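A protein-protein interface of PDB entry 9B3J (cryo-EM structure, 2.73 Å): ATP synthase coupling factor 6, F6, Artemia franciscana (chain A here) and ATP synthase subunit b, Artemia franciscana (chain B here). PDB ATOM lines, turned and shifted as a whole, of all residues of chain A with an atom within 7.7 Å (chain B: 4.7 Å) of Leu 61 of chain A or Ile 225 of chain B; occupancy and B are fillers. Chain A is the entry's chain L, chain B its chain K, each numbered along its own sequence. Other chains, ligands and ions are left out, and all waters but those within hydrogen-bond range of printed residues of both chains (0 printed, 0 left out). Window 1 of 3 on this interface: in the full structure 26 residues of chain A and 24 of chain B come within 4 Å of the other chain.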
ATOM      1  N   TYR A  39     -16.912 -11.087 -11.629  1.00  0.00           N
ATOM      2  CA  TYR A  39     -16.994 -12.168 -10.651  1.00  0.00           C
ATOM      3  C   TYR A  39     -17.702 -11.715  -9.385  1.00  0.00           C
ATOM      4  O   TYR A  39     -18.446 -12.491  -8.779  1.00  0.00           O
ATOM      5  CB  TYR A  39     -15.599 -12.692 -10.316  1.00  0.00           C
ATOM      6  CG  TYR A  39     -15.613 -13.842  -9.334  1.00  0.00           C
ATOM      7  CD1 TYR A  39     -15.925 -15.129  -9.751  1.00  0.00           C
ATOM      8  CD2 TYR A  39     -15.316 -13.644  -7.990  1.00  0.00           C
ATOM      9  CE1 TYR A  39     -15.942 -16.185  -8.863  1.00  0.00           C
ATOM     10  CE2 TYR A  39     -15.335 -14.696  -7.092  1.00  0.00           C
ATOM     11  CZ  TYR A  39     -15.645 -15.965  -7.537  1.00  0.00           C
ATOM     12  OH  TYR A  39     -15.664 -17.019  -6.653  1.00  0.00           O
ATOM     13  N   LEU A  50     -19.489 -20.401  -3.882  1.00  0.00           N
ATOM     14  CA  LEU A  50     -18.345 -20.655  -4.746  1.00  0.00           C
ATOM     15  C   LEU A  50     -18.810 -20.820  -6.187  1.00  0.00           C
ATOM     16  O   LEU A  50     -19.761 -21.559  -6.464  1.00  0.00           O
ATOM     17  CB  LEU A  50     -17.597 -21.901  -4.280  1.00  0.00           C
ATOM     18  CG  LEU A  50     -17.223 -21.944  -2.796  1.00  0.00           C
ATOM     19  CD1 LEU A  50     -16.421 -23.199  -2.480  1.00  0.00           C
ATOM     20  CD2 LEU A  50     -16.457 -20.695  -2.385  1.00  0.00           C
ATOM     21  N   ALA A  53     -16.011 -23.720  -8.934  1.00  0.00           N
ATOM     22  CA  ALA A  53     -14.821 -24.253  -8.290  1.00  0.00           C
ATOM     23  C   ALA A  53     -14.525 -25.665  -8.787  1.00  0.00           C
ATOM     24  O   ALA A  53     -15.427 -26.422  -9.154  1.00  0.00           O
ATOM     25  CB  ALA A  53     -14.989 -24.255  -6.771  1.00  0.00           C
ATOM     26  N   THR A  55     -13.040 -29.644  -8.522  1.00  0.00           N
ATOM     27  CA  THR A  55     -13.377 -30.719  -7.595  1.00  0.00           C
ATOM     28  C   THR A  55     -12.326 -30.864  -6.499  1.00  0.00           C
ATOM     29  O   THR A  55     -12.666 -31.131  -5.341  1.00  0.00           O
ATOM     30  CB  THR A  55     -13.542 -32.032  -8.361  1.00  0.00           C
ATOM     31  OG1 THR A  55     -14.388 -31.815  -9.497  1.00  0.00           O
ATOM     32  CG2 THR A  55     -14.169 -33.100  -7.475  1.00  0.00           C
ATOM     33  N   GLU A  56     -11.048 -30.677  -6.842  1.00  0.00           N
ATOM     34  CA  GLU A  56      -9.974 -30.899  -5.875  1.00  0.00           C
ATOM     35  C   GLU A  56      -9.981 -29.845  -4.773  1.00  0.00           C
ATOM     36  O   GLU A  56      -9.679 -30.151  -3.615  1.00  0.00           O
ATOM     37  CB  GLU A  56      -8.625 -30.920  -6.592  1.00  0.00           C
ATOM     38  CG  GLU A  56      -8.510 -32.006  -7.652  1.00  0.00           C
ATOM     39  CD  GLU A  56      -7.134 -32.070  -8.281  1.00  0.00           C
ATOM     40  OE1 GLU A  56      -6.202 -31.433  -7.749  1.00  0.00           O
ATOM     41  OE2 GLU A  56      -6.984 -32.759  -9.312  1.00  0.00           O
ATOM     42  N   ILE A  57     -10.329 -28.602  -5.116  1.00  0.00           N
ATOM     43  CA  ILE A  57     -10.440 -27.548  -4.110  1.00  0.00           C
ATOM     44  C   ILE A  57     -11.600 -27.833  -3.164  1.00  0.00           C
ATOM     45  O   ILE A  57     -11.490 -27.635  -1.948  1.00  0.00           O
ATOM     46  CB  ILE A  57     -10.582 -26.176  -4.795  1.00  0.00           C
ATOM     47  CG1 ILE A  57      -9.349 -25.885  -5.650  1.00  0.00           C
ATOM     48  CG2 ILE A  57     -10.781 -25.068  -3.772  1.00  0.00           C
ATOM     49  CD1 ILE A  57      -9.420 -24.570  -6.397  1.00  0.00           C
ATOM     50  N   GLN A  58     -12.724 -28.311  -3.706  1.00  0.00           N
ATOM     51  CA  GLN A  58     -13.861 -28.691  -2.873  1.00  0.00           C
ATOM     52  C   GLN A  58     -13.512 -29.858  -1.955  1.00  0.00           C
ATOM     53  O   GLN A  58     -13.900 -29.872  -0.779  1.00  0.00           O
ATOM     54  CB  GLN A  58     -15.056 -29.041  -3.759  1.00  0.00           C
ATOM     55  CG  GLN A  58     -16.283 -29.516  -3.005  1.00  0.00           C
ATOM     56  CD  GLN A  58     -16.975 -28.400  -2.255  1.00  0.00           C
ATOM     57  OE1 GLN A  58     -16.802 -27.222  -2.569  1.00  0.00           O
ATOM     58  NE2 GLN A  58     -17.768 -28.764  -1.255  1.00  0.00           N
ATOM     59  N   ARG A  59     -12.770 -30.841  -2.474  1.00  0.00           N
ATOM     60  CA  ARG A  59     -12.347 -31.974  -1.657  1.00  0.00           C
ATOM     61  C   ARG A  59     -11.402 -31.538  -0.544  1.00  0.00           C
ATOM     62  O   ARG A  59     -11.521 -32.000   0.596  1.00  0.00           O
ATOM     63  CB  ARG A  59     -11.678 -33.035  -2.530  1.00  0.00           C
ATOM     64  CG  ARG A  59     -12.613 -33.777  -3.472  1.00  0.00           C
ATOM     65  CD  ARG A  59     -11.824 -34.755  -4.334  1.00  0.00           C
ATOM     66  NE  ARG A  59     -12.641 -35.407  -5.350  1.00  0.00           N
ATOM     67  CZ  ARG A  59     -12.173 -36.261  -6.251  1.00  0.00           C
ATOM     68  NH1 ARG A  59     -10.893 -36.592  -6.289  1.00  0.00           N
ATOM     69  NH2 ARG A  59     -13.010 -36.796  -7.136  1.00  0.00           N
ATOM     70  N   GLU A  60     -10.455 -30.649  -0.858  1.00  0.00           N
ATOM     71  CA  GLU A  60      -9.525 -30.164   0.157  1.00  0.00           C
ATOM     72  C   GLU A  60     -10.241 -29.324   1.208  1.00  0.00           C
ATOM     73  O   GLU A  60      -9.909 -29.396   2.397  1.00  0.00           O
ATOM     74  CB  GLU A  60      -8.400 -29.366  -0.503  1.00  0.00           C
ATOM     75  CG  GLU A  60      -7.278 -28.963   0.440  1.00  0.00           C
ATOM     76  CD  GLU A  60      -6.131 -28.279  -0.276  1.00  0.00           C
ATOM     77  OE1 GLU A  60      -6.212 -28.113  -1.512  1.00  0.00           O
ATOM     78  OE2 GLU A  60      -5.145 -27.908   0.394  1.00  0.00           O
ATOM     79  N   LEU A  61     -11.231 -28.527   0.789  1.00  0.00           N
ATOM     80  CA  LEU A  61     -12.030 -27.758   1.739  1.00  0.00           C
ATOM     81  C   LEU A  61     -12.817 -28.673   2.670  1.00  0.00           C
ATOM     82  O   LEU A  61     -12.880 -28.429   3.882  1.00  0.00           O
ATOM     83  CB  LEU A  61     -12.976 -26.819   0.990  1.00  0.00           C
ATOM     84  CG  LEU A  61     -14.151 -26.219   1.771  1.00  0.00           C
ATOM     85  CD1 LEU A  61     -13.684 -25.298   2.893  1.00  0.00           C
ATOM     86  CD2 LEU A  61     -15.097 -25.483   0.833  1.00  0.00           C
ATOM     87  N   ASP A  62     -13.419 -29.732   2.122  1.00  0.00           N
ATOM     88  CA  ASP A  62     -14.164 -30.670   2.957  1.00  0.00           C
ATOM     89  C   ASP A  62     -13.241 -31.428   3.903  1.00  0.00           C
ATOM     90  O   ASP A  62     -13.596 -31.673   5.064  1.00  0.00           O
ATOM     91  CB  ASP A  62     -14.953 -31.637   2.078  1.00  0.00           C
ATOM     92  CG  ASP A  62     -16.017 -30.936   1.257  1.00  0.00           C
ATOM     93  OD1 ASP A  62     -16.589 -29.942   1.751  1.00  0.00           O
ATOM     94  OD2 ASP A  62     -16.278 -31.377   0.118  1.00  0.00           O
ATOM     95  N   ALA A  63     -12.048 -31.795   3.429  1.00  0.00           N
ATOM     96  CA  ALA A  63     -11.085 -32.487   4.280  1.00  0.00           C
ATOM     97  C   ALA A  63     -10.599 -31.594   5.414  1.00  0.00           C
ATOM     98  O   ALA A  63     -10.484 -32.045   6.559  1.00  0.00           O
ATOM     99  CB  ALA A  63      -9.905 -32.976   3.442  1.00  0.00           C
ATOM    100  N   GLU A  64     -10.315 -30.323   5.117  1.00  0.00           N
ATOM    101  CA  GLU A  64      -9.859 -29.405   6.154  1.00  0.00           C
ATOM    102  C   GLU A  64     -10.966 -29.100   7.155  1.00  0.00           C
ATOM    103  O   GLU A  64     -10.703 -28.991   8.358  1.00  0.00           O
ATOM    104  CB  GLU A  64      -9.331 -28.117   5.524  1.00  0.00           C
ATOM    105  CG  GLU A  64      -7.999 -28.278   4.810  1.00  0.00           C
ATOM    106  CD  GLU A  64      -6.874 -28.669   5.750  1.00  0.00           C
ATOM    107  OE1 GLU A  64      -6.880 -28.213   6.912  1.00  0.00           O
ATOM    108  OE2 GLU A  64      -5.984 -29.436   5.326  1.00  0.00           O
ATOM    109  N   LEU A  65     -12.208 -28.961   6.678  1.00  0.00           N
ATOM    110  CA  LEU A  65     -13.326 -28.724   7.587  1.00  0.00           C
ATOM    111  C   LEU A  65     -13.568 -29.919   8.497  1.00  0.00           C
ATOM    112  O   LEU A  65     -13.855 -29.751   9.688  1.00  0.00           O
ATOM    113  CB  LEU A  65     -14.589 -28.395   6.795  1.00  0.00           C
ATOM    114  CG  LEU A  65     -14.686 -26.979   6.228  1.00  0.00           C
ATOM    115  CD1 LEU A  65     -15.998 -26.798   5.485  1.00  0.00           C
ATOM    116  CD2 LEU A  65     -14.541 -25.943   7.332  1.00  0.00           C
ATOM    117  N   ASP A  66     -13.448 -31.135   7.956  1.00  0.00           N
ATOM    118  CA  ASP A  66     -13.597 -32.328   8.782  1.00  0.00           C
ATOM    119  C   ASP A  66     -12.458 -32.454   9.788  1.00  0.00           C
ATOM    120  O   ASP A  66     -12.682 -32.842  10.942  1.00  0.00           O
ATOM    121  CB  ASP A  66     -13.668 -33.568   7.892  1.00  0.00           C
ATOM    122  CG  ASP A  66     -14.154 -34.795   8.636  1.00  0.00           C
ATOM    123  OD1 ASP A  66     -14.659 -34.652   9.770  1.00  0.00           O
ATOM    124  OD2 ASP A  66     -14.031 -35.908   8.083  1.00  0.00           O
ATOM    125  N   LYS A  67     -11.229 -32.131   9.368  1.00  0.00           N
ATOM    126  CA  LYS A  67     -10.086 -32.210  10.271  1.00  0.00           C
ATOM    127  C   LYS A  67     -10.199 -31.200  11.404  1.00  0.00           C
ATOM    128  O   LYS A  67      -9.880 -31.512  12.556  1.00  0.00           O
ATOM    129  CB  LYS A  67      -8.791 -31.999   9.490  1.00  0.00           C
ATOM    130  CG  LYS A  67      -7.533 -32.152  10.321  1.00  0.00           C
ATOM    131  CD  LYS A  67      -6.293 -32.068   9.451  1.00  0.00           C
ATOM    132  CE  LYS A  67      -5.038 -32.314  10.265  1.00  0.00           C
ATOM    133  NZ  LYS A  67      -4.857 -31.284  11.319  1.00  0.00           N
ATOM    134  N   LEU A  68     -10.656 -29.984  11.098  1.00  0.00           N
ATOM    135  CA  LEU A  68     -10.843 -28.984  12.144  1.00  0.00           C
ATOM    136  C   LEU A  68     -12.017 -29.337  13.049  1.00  0.00           C
ATOM    137  O   LEU A  68     -11.977 -29.062  14.254  1.00  0.00           O
ATOM    138  CB  LEU A  68     -11.040 -27.602  11.524  1.00  0.00           C
ATOM    139  CG  LEU A  68      -9.815 -27.005  10.832  1.00  0.00           C
ATOM    140  CD1 LEU A  68     -10.122 -25.609  10.315  1.00  0.00           C
ATOM    141  CD2 LEU A  68      -8.620 -26.986  11.772  1.00  0.00           C
ATOM    142  N   ALA B 221     -10.619 -20.408   6.628  1.00  0.00           N
ATOM    143  CA  ALA B 221     -10.572 -21.481   5.642  1.00  0.00           C
ATOM    144  C   ALA B 221     -11.523 -21.213   4.482  1.00  0.00           C
ATOM    145  O   ALA B 221     -11.167 -21.439   3.317  1.00  0.00           O
ATOM    146  CB  ALA B 221     -10.896 -22.816   6.306  1.00  0.00           C
ATOM    147  N   GLN B 222     -12.738 -20.732   4.780  1.00  0.00           N
ATOM    148  CA  GLN B 222     -13.682 -20.399   3.716  1.00  0.00           C
ATOM    149  C   GLN B 222     -13.182 -19.236   2.867  1.00  0.00           C
ATOM    150  O   GLN B 222     -13.367 -19.231   1.645  1.00  0.00           O
ATOM    151  CB  GLN B 222     -15.054 -20.078   4.305  1.00  0.00           C
ATOM    152  CG  GLN B 222     -15.786 -21.281   4.875  1.00  0.00           C
ATOM    153  CD  GLN B 222     -17.179 -20.933   5.362  1.00  0.00           C
ATOM    154  OE1 GLN B 222     -17.676 -19.833   5.122  1.00  0.00           O
ATOM    155  NE2 GLN B 222     -17.818 -21.872   6.052  1.00  0.00           N
ATOM    156  N   ARG B 223     -12.547 -18.242   3.498  1.00  0.00           N
ATOM    157  CA  ARG B 223     -11.970 -17.128   2.753  1.00  0.00           C
ATOM    158  C   ARG B 223     -10.829 -17.590   1.853  1.00  0.00           C
ATOM    159  O   ARG B 223     -10.717 -17.139   0.708  1.00  0.00           O
ATOM    160  CB  ARG B 223     -11.486 -16.050   3.723  1.00  0.00           C
ATOM    161  CG  ARG B 223     -10.893 -14.820   3.056  1.00  0.00           C
ATOM    162  CD  ARG B 223     -10.317 -13.862   4.089  1.00  0.00           C
ATOM    163  NE  ARG B 223     -11.322 -13.426   5.052  1.00  0.00           N
ATOM    164  CZ  ARG B 223     -11.079 -12.618   6.076  1.00  0.00           C
ATOM    165  NH1 ARG B 223      -9.868 -12.136   6.304  1.00  0.00           N
ATOM    166  NH2 ARG B 223     -12.075 -12.287   6.892  1.00  0.00           N
ATOM    167  N   GLN B 224      -9.976 -18.490   2.356  1.00  0.00           N
ATOM    168  CA  GLN B 224      -8.876 -19.016   1.552  1.00  0.00           C
ATOM    169  C   GLN B 224      -9.389 -19.822   0.365  1.00  0.00           C
ATOM    170  O   GLN B 224      -8.867 -19.701  -0.752  1.00  0.00           O
ATOM    171  CB  GLN B 224      -7.962 -19.876   2.422  1.00  0.00           C
ATOM    172  CG  GLN B 224      -6.861 -20.586   1.653  1.00  0.00           C
ATOM    173  CD  GLN B 224      -6.158 -21.639   2.482  1.00  0.00           C
ATOM    174  OE1 GLN B 224      -6.525 -21.888   3.629  1.00  0.00           O
ATOM    175  NE2 GLN B 224      -5.141 -22.265   1.903  1.00  0.00           N
ATOM    176  N   ILE B 225     -10.415 -20.646   0.589  1.00  0.00           N
ATOM    177  CA  ILE B 225     -11.005 -21.424  -0.498  1.00  0.00           C
ATOM    178  C   ILE B 225     -11.668 -20.505  -1.520  1.00  0.00           C
ATOM    179  O   ILE B 225     -11.545 -20.715  -2.739  1.00  0.00           O
ATOM    180  CB  ILE B 225     -11.983 -22.464   0.079  1.00  0.00           C
ATOM    181  CG1 ILE B 225     -11.204 -23.555   0.816  1.00  0.00           C
ATOM    182  CG2 ILE B 225     -12.855 -23.077  -1.010  1.00  0.00           C
ATOM    183  CD1 ILE B 225     -10.217 -24.306  -0.059  1.00  0.00           C
ATOM    184  N   LYS B 226     -12.362 -19.463  -1.045  1.00  0.00           N
ATOM    185  CA  LYS B 226     -12.980 -18.501  -1.952  1.00  0.00           C
ATOM    186  C   LYS B 226     -11.934 -17.772  -2.785  1.00  0.00           C
ATOM    187  O   LYS B 226     -12.113 -17.593  -3.997  1.00  0.00           O
ATOM    188  CB  LYS B 226     -13.825 -17.498  -1.167  1.00  0.00           C
ATOM    189  CG  LYS B 226     -14.465 -16.434  -2.045  1.00  0.00           C
ATOM    190  CD  LYS B 226     -15.191 -15.385  -1.227  1.00  0.00           C
ATOM    191  CE  LYS B 226     -15.759 -14.294  -2.118  1.00  0.00           C
ATOM    192  NZ  LYS B 226     -16.428 -13.225  -1.329  1.00  0.00           N
ATOM    193  N   GLN B 227     -10.820 -17.379  -2.161  1.00  0.00           N
ATOM    194  CA  GLN B 227      -9.741 -16.722  -2.894  1.00  0.00           C
ATOM    195  C   GLN B 227      -9.125 -17.651  -3.935  1.00  0.00           C
ATOM    196  O   GLN B 227      -8.827 -17.224  -5.057  1.00  0.00           O
ATOM    197  CB  GLN B 227      -8.665 -16.229  -1.927  1.00  0.00           C
ATOM    198  CG  GLN B 227      -9.051 -15.001  -1.126  1.00  0.00           C
ATOM    199  CD  GLN B 227      -8.013 -14.641  -0.079  1.00  0.00           C
ATOM    200  OE1 GLN B 227      -7.119 -15.431   0.223  1.00  0.00           O
ATOM    201  NE2 GLN B 227      -8.127 -13.442   0.480  1.00  0.00           N
ATOM    202  N   LYS B 228      -8.941 -18.927  -3.584  1.00  0.00           N
ATOM    203  CA  LYS B 228      -8.274 -19.857  -4.492  1.00  0.00           C
ATOM    204  C   LYS B 228      -9.127 -20.149  -5.723  1.00  0.00           C
ATOM    205  O   LYS B 228      -8.627 -20.123  -6.860  1.00  0.00           O
ATOM    206  CB  LYS B 228      -7.928 -21.149  -3.754  1.00  0.00           C
ATOM    207  CG  LYS B 228      -7.007 -22.070  -4.536  1.00  0.00           C
ATOM    208  CD  LYS B 228      -6.561 -23.255  -3.696  1.00  0.00           C
ATOM    209  CE  LYS B 228      -5.613 -24.155  -4.474  1.00  0.00           C
ATOM    210  NZ  LYS B 228      -5.178 -25.330  -3.670  1.00  0.00           N
ATOM    211  N   ASN B 229     -10.425 -20.414  -5.526  1.00  0.00           N
ATOM    212  CA  ASN B 229     -11.268 -20.693  -6.687  1.00  0.00           C
ATOM    213  C   ASN B 229     -11.563 -19.430  -7.488  1.00  0.00           C
ATOM    214  O   ASN B 229     -11.760 -19.512  -8.707  1.00  0.00           O
ATOM    215  CB  ASN B 229     -12.570 -21.384  -6.276  1.00  0.00           C
ATOM    216  CG  ASN B 229     -13.381 -20.581  -5.279  1.00  0.00           C
ATOM    217  OD1 ASN B 229     -13.921 -19.521  -5.599  1.00  0.00           O
ATOM    218  ND2 ASN B 229     -13.503 -21.108  -4.069  1.00  0.00           N
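Of the printed residues of chain B, Leu 50 of chain A touches Ile 225 (3.9 Å) and Asn 229 (3.4 Å). Printed residues of chain B within 4 Å of Ala 53 of chain A: Asn 229. Printed residues of chain B within 4 Å of Ile 57 of chain A: Ile 225 (3.8 Å) and Lys 228 (3.9 Å). Leu 61 of chain A touches one residue of chain B. Of chain A, only Leu 50, Ile 57 and Leu 61 come within 4 Å of Ile 225 of chain B. Printed residues of chain A within 4 Å of Lys 228 of chain B: Ile 57 and Glu 60. The nearest residue of chain B that does not touch Leu 61 of chain A is Ala 221 of chain B (4.6 Å). The nearest residue of chain A that does not touch Ile 225 of chain B is Glu 60 of chain A (5.2 Å). The nearest printed residue of chain B that does not touch Tyr 39 of chain A is Lys 226 of chain B (4.5 Å).
Hydrophobic or aromatic side chains of chain B within 4 Å of the printed part of chain A: Ile 225. Of the 17 printed residues of chain A, 6 touch a printed residue of chain B. Printed residues of chain A that touch a printed residue of chain B: Tyr 39, Leu 50, Ala 53, Ile 57, Glu 60 and Leu 61. Hydrophobic or aromatic side chains of chain A that line the printed part of chain B: Tyr 39, Leu 50, Ala 53, Ile 57 and Leu 61.
The side-chain carboxylate of Glu 60 of chain A is in salt-bridge range of the side-chain amino group of Lys 228 of chain B, at 3.7 Å. OD1 of Asn 229 of chain B is in hydrogen-bond range of OH of Tyr 39 of chain A, at 3.2 Å.
Among the printed residues, pairs that only touch across the chains: Leu 50 of chain A with Asn 229 of chain B (3.4 Å), Leu 61 of chain A with Ile 225 of chain B (3.7 Å), Ala 53 of chain A with Asn 229 of chain B (3.8 Å), Ile 57 of chain A with Ile 225 of chain B (3.8 Å), Leu 50 of chain A with Ile 225 of chain B (3.9 Å) and Ile 57 of chain A with Lys 228 of chain B (3.9 Å).
The side-chain amide oxygen (OD1) of Asn 229 of chain B sits close to the backbone carbonyl oxygen (O) of Lys 226 of chain B, 3.1 Å away.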
